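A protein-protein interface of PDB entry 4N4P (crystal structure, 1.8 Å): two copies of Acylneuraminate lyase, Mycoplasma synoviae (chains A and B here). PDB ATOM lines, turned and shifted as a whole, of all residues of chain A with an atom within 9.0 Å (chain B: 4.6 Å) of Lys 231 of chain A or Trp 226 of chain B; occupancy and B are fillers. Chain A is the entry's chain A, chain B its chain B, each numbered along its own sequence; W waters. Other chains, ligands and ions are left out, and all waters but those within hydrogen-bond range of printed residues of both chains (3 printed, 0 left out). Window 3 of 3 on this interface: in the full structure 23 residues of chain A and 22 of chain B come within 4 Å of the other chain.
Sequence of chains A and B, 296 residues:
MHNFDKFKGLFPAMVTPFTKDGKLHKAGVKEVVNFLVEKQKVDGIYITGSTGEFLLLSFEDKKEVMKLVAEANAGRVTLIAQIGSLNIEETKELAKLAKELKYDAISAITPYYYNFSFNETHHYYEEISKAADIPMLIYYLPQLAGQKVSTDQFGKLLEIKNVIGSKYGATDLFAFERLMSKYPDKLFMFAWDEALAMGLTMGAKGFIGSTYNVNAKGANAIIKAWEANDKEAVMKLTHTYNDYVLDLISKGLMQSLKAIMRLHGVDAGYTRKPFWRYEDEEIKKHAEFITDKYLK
OG1 of Thr 201 of chain B lies within hydrogen-bond range of OG1 of Thr 201 of chain A (3.0 Å).
The side-chain amino group of Lys 231 of chain A lies close to the backbone carbonyl oxygen of Trp 226 of chain B (3.1 Å).
The side-chain amino group (NZ) of Lys 231 of chain A lies within hydrogen-bond range of the side-chain amide oxygen (OD1) of Asn 229 of chain B (2.6 Å).
Hydrophobic or aromatic side chains of chain B within 4 Å of the printed part of chain A: Trp 226.
Along chain B the printed residues that touch a printed residue of chain A span positions 200 to 229.
Of the 20 printed residues of chain A, 5 touch a printed residue of chain B.
Hydrophobic or aromatic side chains of chain A within 4 Å of the printed part of chain B: Met 235.
Of chain B, only Trp 226 and Asn 229 come within 4 Å of Lys 231 of chain A.
Trp 226 of chain B touches one residue of chain A.
No residue of chain A comes within 4 Å of Ala 225 of chain B.
Of the printed residues of chain B, Met 235 of chain A touches Leu 200 (3.8 Å) and Thr 201 (3.4 Å).
Printed residues of chain B within 4 Å of Ala 197 of chain A: Thr 201.
Of the printed residues of chain B, Asn 229 of chain A touches Asn 229.
Met 202 of chain A touches none of the printed residues of chain B.
The nearest printed residue of chain B that does not touch Asn 229 of chain A is Ala 228 of chain B (6.4 Å).
The backbone carbonyl oxygen (O) of Ala 197 of chain A lies within hydrogen-bond range of the side-chain hydroxyl (OG1) of Thr 201 of chain A (2.8 Å).
The side-chain hydroxyl of Thr 201 of chain A sits at hydrogen-bond distance from the indole nitrogen of Trp 226 of chain A.
Water W2 lies within hydrogen-bond range of O of Thr 201 of chain B (2.8 Å) and O of Lys 231 of chain A (2.9 Å).
Water W1 lies within hydrogen-bond range of the side-chain hydroxyl of Thr 201 of chain A, the indole nitrogen of Trp 226 of chain B, the side-chain hydroxyl of Thr 201 of chain B and the indole nitrogen of Trp 226 of chain A.
Water W3 bridges NZ of Lys 231 of chain A (3.1 Å) and O of Glu 227 of chain B (3.2 Å).
Among the printed residues, merely in contact across the chains: Ala 197 of chain A with Thr 201 of chain B (3.9 Å), Asn 229 of chain A with Asn 229 of chain B (3.4 Å), Met 235 of chain A with Leu 200 of chain B (3.8 Å) and Met 235 of chain A with Thr 201 of chain B (3.4 Å).
Thr 201 of chain B touches its own counterpart, Thr 201 of chain A.
Asn 229 of chain A touches its own counterpart, Asn 229 of chain B.
Of the 7 pairs that touch across the chains among the printed residues, 2 have their exchanged pair printed and touching as well.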
ATOM      1  N   ALA A 197     -16.923  11.357 -33.817  1.00  0.00           N
ATOM      2  CA  ALA A 197     -17.055  10.510 -32.632  1.00  0.00           C
ATOM      3  C   ALA A 197     -15.836   9.613 -32.451  1.00  0.00           C
ATOM      4  O   ALA A 197     -15.431   9.322 -31.329  1.00  0.00           O
ATOM      5  CB  ALA A 197     -18.325   9.686 -32.707  1.00  0.00           C
ATOM      6  N   THR A 201     -13.386   9.747 -29.178  1.00  0.00           N
ATOM      7  CA  THR A 201     -13.028   8.493 -28.514  1.00  0.00           C
ATOM      8  C   THR A 201     -11.514   8.377 -28.281  1.00  0.00           C
ATOM      9  O   THR A 201     -11.084   7.798 -27.295  1.00  0.00           O
ATOM     10  CB  THR A 201     -13.591   7.290 -29.285  1.00  0.00           C
ATOM     11  OG1 THR A 201     -15.028   7.400 -29.292  1.00  0.00           O
ATOM     12  CG2 THR A 201     -13.193   5.963 -28.591  1.00  0.00           C
ATOM     13  N   MET A 202     -10.712   8.954 -29.171  1.00  0.00           N
ATOM     14  CA  MET A 202      -9.273   8.931 -28.956  1.00  0.00           C
ATOM     15  C   MET A 202      -8.711  10.236 -28.338  1.00  0.00           C
ATOM     16  O   MET A 202      -7.483  10.440 -28.302  1.00  0.00           O
ATOM     17  CB  MET A 202      -8.529   8.482 -30.230  1.00  0.00           C
ATOM     18  CG  MET A 202      -7.204   7.725 -29.913  1.00  0.00           C
ATOM     19  SD  MET A 202      -7.290   6.535 -28.539  1.00  0.00           S
ATOM     20  CE  MET A 202      -8.719   5.482 -28.914  1.00  0.00           C
ATOM     21  N   ILE A 222     -23.752  14.983 -31.361  1.00  0.00           N
ATOM     22  CA  ILE A 222     -22.839  13.830 -31.238  1.00  0.00           C
ATOM     23  C   ILE A 222     -21.934  14.008 -30.006  1.00  0.00           C
ATOM     24  O   ILE A 222     -21.795  13.101 -29.187  1.00  0.00           O
ATOM     25  CB  ILE A 222     -21.981  13.625 -32.505  1.00  0.00           C
ATOM     26  CG1 ILE A 222     -22.861  13.221 -33.699  1.00  0.00           C
ATOM     27  CG2 ILE A 222     -20.920  12.537 -32.283  1.00  0.00           C
ATOM     28  CD1 ILE A 222     -22.149  13.460 -35.013  1.00  0.00           C
ATOM     29  N   LYS A 224     -22.438  15.864 -27.358  1.00  0.00           N
ATOM     30  CA  LYS A 224     -23.237  15.773 -26.109  1.00  0.00           C
ATOM     31  C   LYS A 224     -23.605  14.324 -25.787  1.00  0.00           C
ATOM     32  O   LYS A 224     -23.501  13.896 -24.630  1.00  0.00           O
ATOM     33  CB  LYS A 224     -24.471  16.674 -26.155  1.00  0.00           C
ATOM     34  CG  LYS A 224     -24.129  18.179 -26.266  1.00  0.00           C
ATOM     35  CD  LYS A 224     -23.070  18.674 -25.236  1.00  0.00           C
ATOM     36  CE  LYS A 224     -23.717  19.077 -23.916  1.00  0.00           C
ATOM     37  NZ  LYS A 224     -22.947  20.151 -23.183  1.00  0.00           N
ATOM     38  N   ALA A 225     -23.995  13.564 -26.803  1.00  0.00           N
ATOM     39  CA  ALA A 225     -24.294  12.133 -26.608  1.00  0.00           C
ATOM     40  C   ALA A 225     -23.063  11.354 -26.133  1.00  0.00           C
ATOM     41  O   ALA A 225     -23.160  10.486 -25.257  1.00  0.00           O
ATOM     42  CB  ALA A 225     -24.882  11.497 -27.920  1.00  0.00           C
ATOM     43  N   TRP A 226     -21.910  11.681 -26.705  1.00  0.00           N
ATOM     44  CA  TRP A 226     -20.656  11.039 -26.338  1.00  0.00           C
ATOM     45  C   TRP A 226     -20.324  11.368 -24.895  1.00  0.00           C
ATOM     46  O   TRP A 226     -20.029  10.456 -24.127  1.00  0.00           O
ATOM     47  CB  TRP A 226     -19.519  11.480 -27.282  1.00  0.00           C
ATOM     48  CG  TRP A 226     -18.254  10.749 -27.046  1.00  0.00           C
ATOM     49  CD1 TRP A 226     -17.890   9.513 -27.548  1.00  0.00           C
ATOM     50  CD2 TRP A 226     -17.194  11.170 -26.209  1.00  0.00           C
ATOM     51  NE1 TRP A 226     -16.645   9.173 -27.090  1.00  0.00           N
ATOM     52  CE2 TRP A 226     -16.189  10.178 -26.272  1.00  0.00           C
ATOM     53  CE3 TRP A 226     -16.969  12.323 -25.438  1.00  0.00           C
ATOM     54  CZ2 TRP A 226     -14.992  10.276 -25.559  1.00  0.00           C
ATOM     55  CZ3 TRP A 226     -15.769  12.426 -24.734  1.00  0.00           C
ATOM     56  CH2 TRP A 226     -14.797  11.403 -24.802  1.00  0.00           C
ATOM     57  N   GLU A 227     -20.400  12.650 -24.514  1.00  0.00           N
ATOM     58  CA  GLU A 227     -20.117  13.045 -23.116  1.00  0.00           C
ATOM     59  C   GLU A 227     -21.103  12.400 -22.136  1.00  0.00           C
ATOM     60  O   GLU A 227     -20.736  12.105 -20.997  1.00  0.00           O
ATOM     61  CB  GLU A 227     -20.150  14.583 -22.956  1.00  0.00           C
ATOM     62  CG  GLU A 227     -19.027  15.270 -23.715  1.00  0.00           C
ATOM     63  CD  GLU A 227     -19.137  16.778 -23.688  1.00  0.00           C
ATOM     64  OE1 GLU A 227     -20.237  17.279 -23.385  1.00  0.00           O
ATOM     65  OE2 GLU A 227     -18.131  17.456 -23.996  1.00  0.00           O
ATOM     66  N   ALA A 228     -22.334  12.183 -22.588  1.00  0.00           N
ATOM     67  CA  ALA A 228     -23.400  11.591 -21.761  1.00  0.00           C
ATOM     68  C   ALA A 228     -23.339  10.063 -21.704  1.00  0.00           C
ATOM     69  O   ALA A 228     -24.157   9.423 -21.016  1.00  0.00           O
ATOM     70  CB  ALA A 228     -24.756  12.022 -22.259  1.00  0.00           C
ATOM     71  N   ASN A 229     -22.377   9.477 -22.414  1.00  0.00           N
ATOM     72  CA  ASN A 229     -22.204   8.020 -22.467  1.00  0.00           C
ATOM     73  C   ASN A 229     -23.388   7.307 -23.103  1.00  0.00           C
ATOM     74  O   ASN A 229     -23.661   6.137 -22.798  1.00  0.00           O
ATOM     75  CB  ASN A 229     -21.905   7.433 -21.064  1.00  0.00           C
ATOM     76  CG  ASN A 229     -20.778   8.143 -20.388  1.00  0.00           C
ATOM     77  OD1 ASN A 229     -19.688   8.246 -20.944  1.00  0.00           O
ATOM     78  ND2 ASN A 229     -21.022   8.653 -19.180  1.00  0.00           N
ATOM     79  N   ASP A 230     -24.077   8.001 -24.000  1.00  0.00           N
ATOM     80  CA  ASP A 230     -25.211   7.412 -24.685  1.00  0.00           C
ATOM     81  C   ASP A 230     -24.651   6.804 -25.974  1.00  0.00           C
ATOM     82  O   ASP A 230     -24.696   7.427 -27.037  1.00  0.00           O
ATOM     83  CB  ASP A 230     -26.262   8.482 -24.958  1.00  0.00           C
ATOM     84  CG  ASP A 230     -27.543   7.908 -25.566  1.00  0.00           C
ATOM     85  OD1 ASP A 230     -27.556   6.754 -26.056  1.00  0.00           O
ATOM     86  OD2 ASP A 230     -28.543   8.643 -25.575  1.00  0.00           O
ATOM     87  N   LYS A 231     -24.110   5.593 -25.853  1.00  0.00           N
ATOM     88  CA  LYS A 231     -23.352   4.965 -26.941  1.00  0.00           C
ATOM     89  C   LYS A 231     -24.190   4.787 -28.186  1.00  0.00           C
ATOM     90  O   LYS A 231     -23.705   4.996 -29.299  1.00  0.00           O
ATOM     91  CB  LYS A 231     -22.863   3.572 -26.543  1.00  0.00           C
ATOM     92  CG  LYS A 231     -22.199   3.453 -25.228  1.00  0.00           C
ATOM     93  CD  LYS A 231     -20.855   4.090 -25.263  1.00  0.00           C
ATOM     94  CE  LYS A 231     -19.992   3.395 -24.236  1.00  0.00           C
ATOM     95  NZ  LYS A 231     -20.719   3.240 -22.950  1.00  0.00           N
ATOM     96  N   GLU A 232     -25.440   4.356 -27.994  1.00  0.00           N
ATOM     97  CA  GLU A 232     -26.354   4.165 -29.108  1.00  0.00           C
ATOM     98  C   GLU A 232     -26.636   5.461 -29.859  1.00  0.00           C
ATOM     99  O   GLU A 232     -26.712   5.440 -31.092  1.00  0.00           O
ATOM    100  CB  GLU A 232     -27.676   3.491 -28.677  1.00  0.00           C
ATOM    101  CG  GLU A 232     -27.487   2.003 -28.279  1.00  0.00           C
ATOM    102  CD  GLU A 232     -27.024   1.128 -29.444  1.00  0.00           C
ATOM    103  OE1 GLU A 232     -27.766   0.992 -30.456  1.00  0.00           O
ATOM    104  OE2 GLU A 232     -25.901   0.581 -29.353  1.00  0.00           O
ATOM    105  N   ALA A 233     -26.810   6.563 -29.118  1.00  0.00           N
ATOM    106  CA  ALA A 233     -27.090   7.863 -29.749  1.00  0.00           C
ATOM    107  C   ALA A 233     -25.882   8.342 -30.531  1.00  0.00           C
ATOM    108  O   ALA A 233     -26.034   8.898 -31.626  1.00  0.00           O
ATOM    109  CB  ALA A 233     -27.524   8.932 -28.706  1.00  0.00           C
ATOM    110  N   VAL A 234     -24.682   8.106 -29.999  1.00  0.00           N
ATOM    111  CA  VAL A 234     -23.464   8.496 -30.733  1.00  0.00           C
ATOM    112  C   VAL A 234     -23.481   7.812 -32.114  1.00  0.00           C
ATOM    113  O   VAL A 234     -23.192   8.437 -33.129  1.00  0.00           O
ATOM    114  CB  VAL A 234     -22.189   8.114 -29.982  1.00  0.00           C
ATOM    115  CG1 VAL A 234     -20.951   8.290 -30.877  1.00  0.00           C
ATOM    116  CG2 VAL A 234     -22.035   8.971 -28.722  1.00  0.00           C
ATOM    117  N   MET A 235     -23.783   6.516 -32.130  1.00  0.00           N
ATOM    118  CA  MET A 235     -23.892   5.777 -33.405  1.00  0.00           C
ATOM    119  C   MET A 235     -24.951   6.350 -34.332  1.00  0.00           C
ATOM    120  O   MET A 235     -24.674   6.612 -35.494  1.00  0.00           O
ATOM    121  CB  MET A 235     -24.202   4.299 -33.162  1.00  0.00           C
ATOM    122  CG  MET A 235     -23.172   3.651 -32.260  1.00  0.00           C
ATOM    123  SD  MET A 235     -23.623   1.954 -31.842  1.00  0.00           S
ATOM    124  CE  MET A 235     -22.633   1.732 -30.354  1.00  0.00           C
ATOM    125  N   LYS A 236     -26.174   6.479 -33.820  1.00  0.00           N
ATOM    126  CA  LYS A 236     -27.305   6.923 -34.625  1.00  0.00           C
ATOM    127  C   LYS A 236     -27.071   8.341 -35.158  1.00  0.00           C
ATOM    128  O   LYS A 236     -27.276   8.595 -36.338  1.00  0.00           O
ATOM    129  CB  LYS A 236     -28.594   6.844 -33.793  1.00  0.00           C
ATOM    130  CG  LYS A 236     -29.830   7.428 -34.494  1.00  0.00           C
ATOM    131  CD  LYS A 236     -31.093   7.326 -33.604  1.00  0.00           C
ATOM    132  CE  LYS A 236     -32.163   8.346 -34.053  1.00  0.00           C
ATOM    133  NZ  LYS A 236     -31.700   9.762 -33.741  1.00  0.00           N
ATOM    134  N   LEU A 237     -26.606   9.244 -34.282  1.00  0.00           N
ATOM    135  CA  LEU A 237     -26.377  10.647 -34.675  1.00  0.00           C
ATOM    136  C   LEU A 237     -25.198  10.786 -35.651  1.00  0.00           C
ATOM    137  O   LEU A 237     -25.170  11.711 -36.485  1.00  0.00           O
ATOM    138  CB  LEU A 237     -26.133  11.545 -33.451  1.00  0.00           C
ATOM    139  CG  LEU A 237     -27.347  11.674 -32.513  1.00  0.00           C
ATOM    140  CD1 LEU A 237     -26.843  12.276 -31.193  1.00  0.00           C
ATOM    141  CD2 LEU A 237     -28.489  12.515 -33.105  1.00  0.00           C
ATOM    142  N   THR A 238     -24.231   9.881 -35.532  1.00  0.00           N
ATOM    143  CA  THR A 238     -23.129   9.850 -36.490  1.00  0.00           C
ATOM    144  C   THR A 238     -23.652   9.381 -37.863  1.00  0.00           C
ATOM    145  O   THR A 238     -23.304   9.971 -38.895  1.00  0.00           O
ATOM    146  CB  THR A 238     -21.994   8.937 -36.020  1.00  0.00           C
ATOM    147  OG1 THR A 238     -21.361   9.534 -34.866  1.00  0.00           O
ATOM    148  CG2 THR A 238     -20.924   8.743 -37.150  1.00  0.00           C
ATOM    149  N   HIS A 239     -24.489   8.340 -37.869  1.00  0.00           N
ATOM    150  CA  HIS A 239     -25.039   7.868 -39.164  1.00  0.00           C
ATOM    151  C   HIS A 239     -25.812   8.986 -39.837  1.00  0.00           C
ATOM    152  O   HIS A 239     -25.642   9.227 -41.031  1.00  0.00           O
ATOM    153  CB  HIS A 239     -25.910   6.617 -38.968  1.00  0.00           C
ATOM    154  CG  HIS A 239     -25.143   5.450 -38.413  1.00  0.00           C
ATOM    155  ND1 HIS A 239     -23.842   5.179 -38.776  1.00  0.00           N
ATOM    156  CD2 HIS A 239     -25.494   4.490 -37.520  1.00  0.00           C
ATOM    157  CE1 HIS A 239     -23.417   4.103 -38.131  1.00  0.00           C
ATOM    158  NE2 HIS A 239     -24.404   3.657 -37.371  1.00  0.00           N
ATOM    159  N   LEU B 200     -15.813  -0.254 -31.668  1.00  0.00           N
ATOM    160  CA  LEU B 200     -16.799  -0.218 -30.581  1.00  0.00           C
ATOM    161  C   LEU B 200     -17.667   1.041 -30.673  1.00  0.00           C
ATOM    162  O   LEU B 200     -18.902   0.975 -30.552  1.00  0.00           O
ATOM    163  CB  LEU B 200     -16.080  -0.226 -29.242  1.00  0.00           C
ATOM    164  CG  LEU B 200     -15.588  -1.554 -28.648  1.00  0.00           C
ATOM    165  CD1 LEU B 200     -14.725  -1.250 -27.435  1.00  0.00           C
ATOM    166  CD2 LEU B 200     -16.710  -2.537 -28.261  1.00  0.00           C
ATOM    167  N   THR B 201     -17.008   2.162 -30.919  1.00  0.00           N
ATOM    168  CA  THR B 201     -17.682   3.456 -31.018  1.00  0.00           C
ATOM    169  C   THR B 201     -18.779   3.435 -32.060  1.00  0.00           C
ATOM    170  O   THR B 201     -19.856   3.997 -31.836  1.00  0.00           O
ATOM    171  CB  THR B 201     -16.684   4.584 -31.364  1.00  0.00           C
ATOM    172  OG1 THR B 201     -15.701   4.616 -30.333  1.00  0.00           O
ATOM    173  CG2 THR B 201     -17.392   5.996 -31.367  1.00  0.00           C
ATOM    174  N   ILE B 222      -9.894  -2.811 -22.829  1.00  0.00           N
ATOM    175  CA  ILE B 222     -10.450  -1.726 -23.628  1.00  0.00           C
ATOM    176  C   ILE B 222     -11.975  -1.856 -23.722  1.00  0.00           C
ATOM    177  O   ILE B 222     -12.705  -0.882 -23.513  1.00  0.00           O
ATOM    178  CB  ILE B 222      -9.854  -1.678 -25.053  1.00  0.00           C
ATOM    179  CG1 ILE B 222      -8.339  -1.441 -24.998  1.00  0.00           C
ATOM    180  CG2 ILE B 222     -10.566  -0.591 -25.902  1.00  0.00           C
ATOM    181  CD1 ILE B 222      -7.640  -1.650 -26.365  1.00  0.00           C
ATOM    182  N   ILE B 223     -12.443  -3.058 -24.011  1.00  0.00           N
ATOM    183  CA  ILE B 223     -13.886  -3.316 -24.092  1.00  0.00           C
ATOM    184  C   ILE B 223     -14.605  -3.007 -22.779  1.00  0.00           C
ATOM    185  O   ILE B 223     -15.640  -2.293 -22.766  1.00  0.00           O
ATOM    186  CB  ILE B 223     -14.181  -4.758 -24.551  1.00  0.00           C
ATOM    187  CG1 ILE B 223     -13.633  -4.958 -25.969  1.00  0.00           C
ATOM    188  CG2 ILE B 223     -15.717  -5.044 -24.491  1.00  0.00           C
ATOM    189  CD1 ILE B 223     -13.686  -6.439 -26.467  1.00  0.00           C
ATOM    190  N   LYS B 224     -14.059  -3.524 -21.680  1.00  0.00           N
ATOM    191  CA  LYS B 224     -14.649  -3.290 -20.356  1.00  0.00           C
ATOM    192  C   LYS B 224     -14.646  -1.808 -19.983  1.00  0.00           C
ATOM    193  O   LYS B 224     -15.662  -1.299 -19.441  1.00  0.00           O
ATOM    194  CB  LYS B 224     -13.897  -4.095 -19.282  1.00  0.00           C
ATOM    195  CG  LYS B 224     -14.284  -5.589 -19.129  1.00  0.00           C
ATOM    196  CD  LYS B 224     -14.776  -6.266 -20.370  1.00  0.00           C
ATOM    197  CE  LYS B 224     -14.647  -7.790 -20.230  1.00  0.00           C
ATOM    198  NZ  LYS B 224     -15.088  -8.468 -21.495  1.00  0.00           N
ATOM    199  N   ALA B 225     -13.540  -1.104 -20.248  1.00  0.00           N
ATOM    200  CA  ALA B 225     -13.513   0.364 -20.010  1.00  0.00           C
ATOM    201  C   ALA B 225     -14.609   1.067 -20.813  1.00  0.00           C
ATOM    202  O   ALA B 225     -15.310   1.942 -20.311  1.00  0.00           O
ATOM    203  CB  ALA B 225     -12.123   0.982 -20.337  1.00  0.00           C
ATOM    204  N   TRP B 226     -14.727   0.697 -22.083  1.00  0.00           N
ATOM    205  CA  TRP B 226     -15.713   1.291 -22.969  1.00  0.00           C
ATOM    206  C   TRP B 226     -17.133   1.059 -22.450  1.00  0.00           C
ATOM    207  O   TRP B 226     -17.929   2.000 -22.385  1.00  0.00           O
ATOM    208  CB  TRP B 226     -15.539   0.740 -24.382  1.00  0.00           C
ATOM    209  CG  TRP B 226     -16.368   1.430 -25.400  1.00  0.00           C
ATOM    210  CD1 TRP B 226     -16.055   2.579 -26.074  1.00  0.00           C
ATOM    211  CD2 TRP B 226     -17.655   1.035 -25.850  1.00  0.00           C
ATOM    212  NE1 TRP B 226     -17.064   2.905 -26.940  1.00  0.00           N
ATOM    213  CE2 TRP B 226     -18.072   1.988 -26.804  1.00  0.00           C
ATOM    214  CE3 TRP B 226     -18.512  -0.038 -25.531  1.00  0.00           C
ATOM    215  CZ2 TRP B 226     -19.298   1.894 -27.475  1.00  0.00           C
ATOM    216  CZ3 TRP B 226     -19.747  -0.126 -26.186  1.00  0.00           C
ATOM    217  CH2 TRP B 226     -20.122   0.840 -27.148  1.00  0.00           C
ATOM    218  N   GLU B 227     -17.431  -0.188 -22.077  1.00  0.00           N
ATOM    219  CA  GLU B 227     -18.726  -0.537 -21.501  1.00  0.00           C
ATOM    220  C   GLU B 227     -19.005   0.189 -20.183  1.00  0.00           C
ATOM    221  O   GLU B 227     -20.158   0.521 -19.879  1.00  0.00           O
ATOM    222  CB  GLU B 227     -18.820  -2.043 -21.287  1.00  0.00           C
ATOM    223  CG  GLU B 227     -18.926  -2.805 -22.609  1.00  0.00           C
ATOM    224  CD  GLU B 227     -18.887  -4.320 -22.457  1.00  0.00           C
ATOM    225  OE1 GLU B 227     -18.388  -4.817 -21.428  1.00  0.00           O
ATOM    226  OE2 GLU B 227     -19.349  -5.011 -23.388  1.00  0.00           O
ATOM    227  N   ALA B 228     -17.946   0.440 -19.431  1.00  0.00           N
ATOM    228  CA  ALA B 228     -18.053   1.054 -18.106  1.00  0.00           C
ATOM    229  C   ALA B 228     -18.071   2.587 -18.206  1.00  0.00           C
ATOM    230  O   ALA B 228     -18.069   3.276 -17.182  1.00  0.00           O
ATOM    231  CB  ALA B 228     -16.904   0.559 -17.223  1.00  0.00           C
ATOM    232  N   ASN B 229     -18.090   3.104 -19.442  1.00  0.00           N
ATOM    233  CA  ASN B 229     -18.050   4.554 -19.705  1.00  0.00           C
ATOM    234  C   ASN B 229     -16.745   5.239 -19.274  1.00  0.00           C
ATOM    235  O   ASN B 229     -16.718   6.457 -19.072  1.00  0.00           O
ATOM    236  CB  ASN B 229     -19.250   5.291 -19.049  1.00  0.00           C
ATOM    237  CG  ASN B 229     -20.606   4.696 -19.422  1.00  0.00           C
ATOM    238  OD1 ASN B 229     -20.790   4.168 -20.509  1.00  0.00           O
ATOM    239  ND2 ASN B 229     -21.583   4.840 -18.523  1.00  0.00           N
ATOM    240  N   VAL B 234     -10.304   4.052 -21.915  1.00  0.00           N
ATOM    241  CA  VAL B 234     -10.357   3.560 -23.295  1.00  0.00           C
ATOM    242  C   VAL B 234      -9.162   4.118 -24.074  1.00  0.00           C
ATOM    243  O   VAL B 234      -8.495   3.389 -24.801  1.00  0.00           O
ATOM    244  CB  VAL B 234     -11.685   3.913 -24.001  1.00  0.00           C
ATOM    245  CG1 VAL B 234     -11.593   3.632 -25.539  1.00  0.00           C
ATOM    246  CG2 VAL B 234     -12.796   3.108 -23.362  1.00  0.00           C
HETATM  247  O   HOH W   1     -16.728   5.769 -27.597  1.00  0.00           O
HETATM  248  O   HOH W   2     -20.838   4.762 -29.337  1.00  0.00           O
HETATM  249  O   HOH W   3     -22.164   0.530 -22.377  1.00  0.00           O
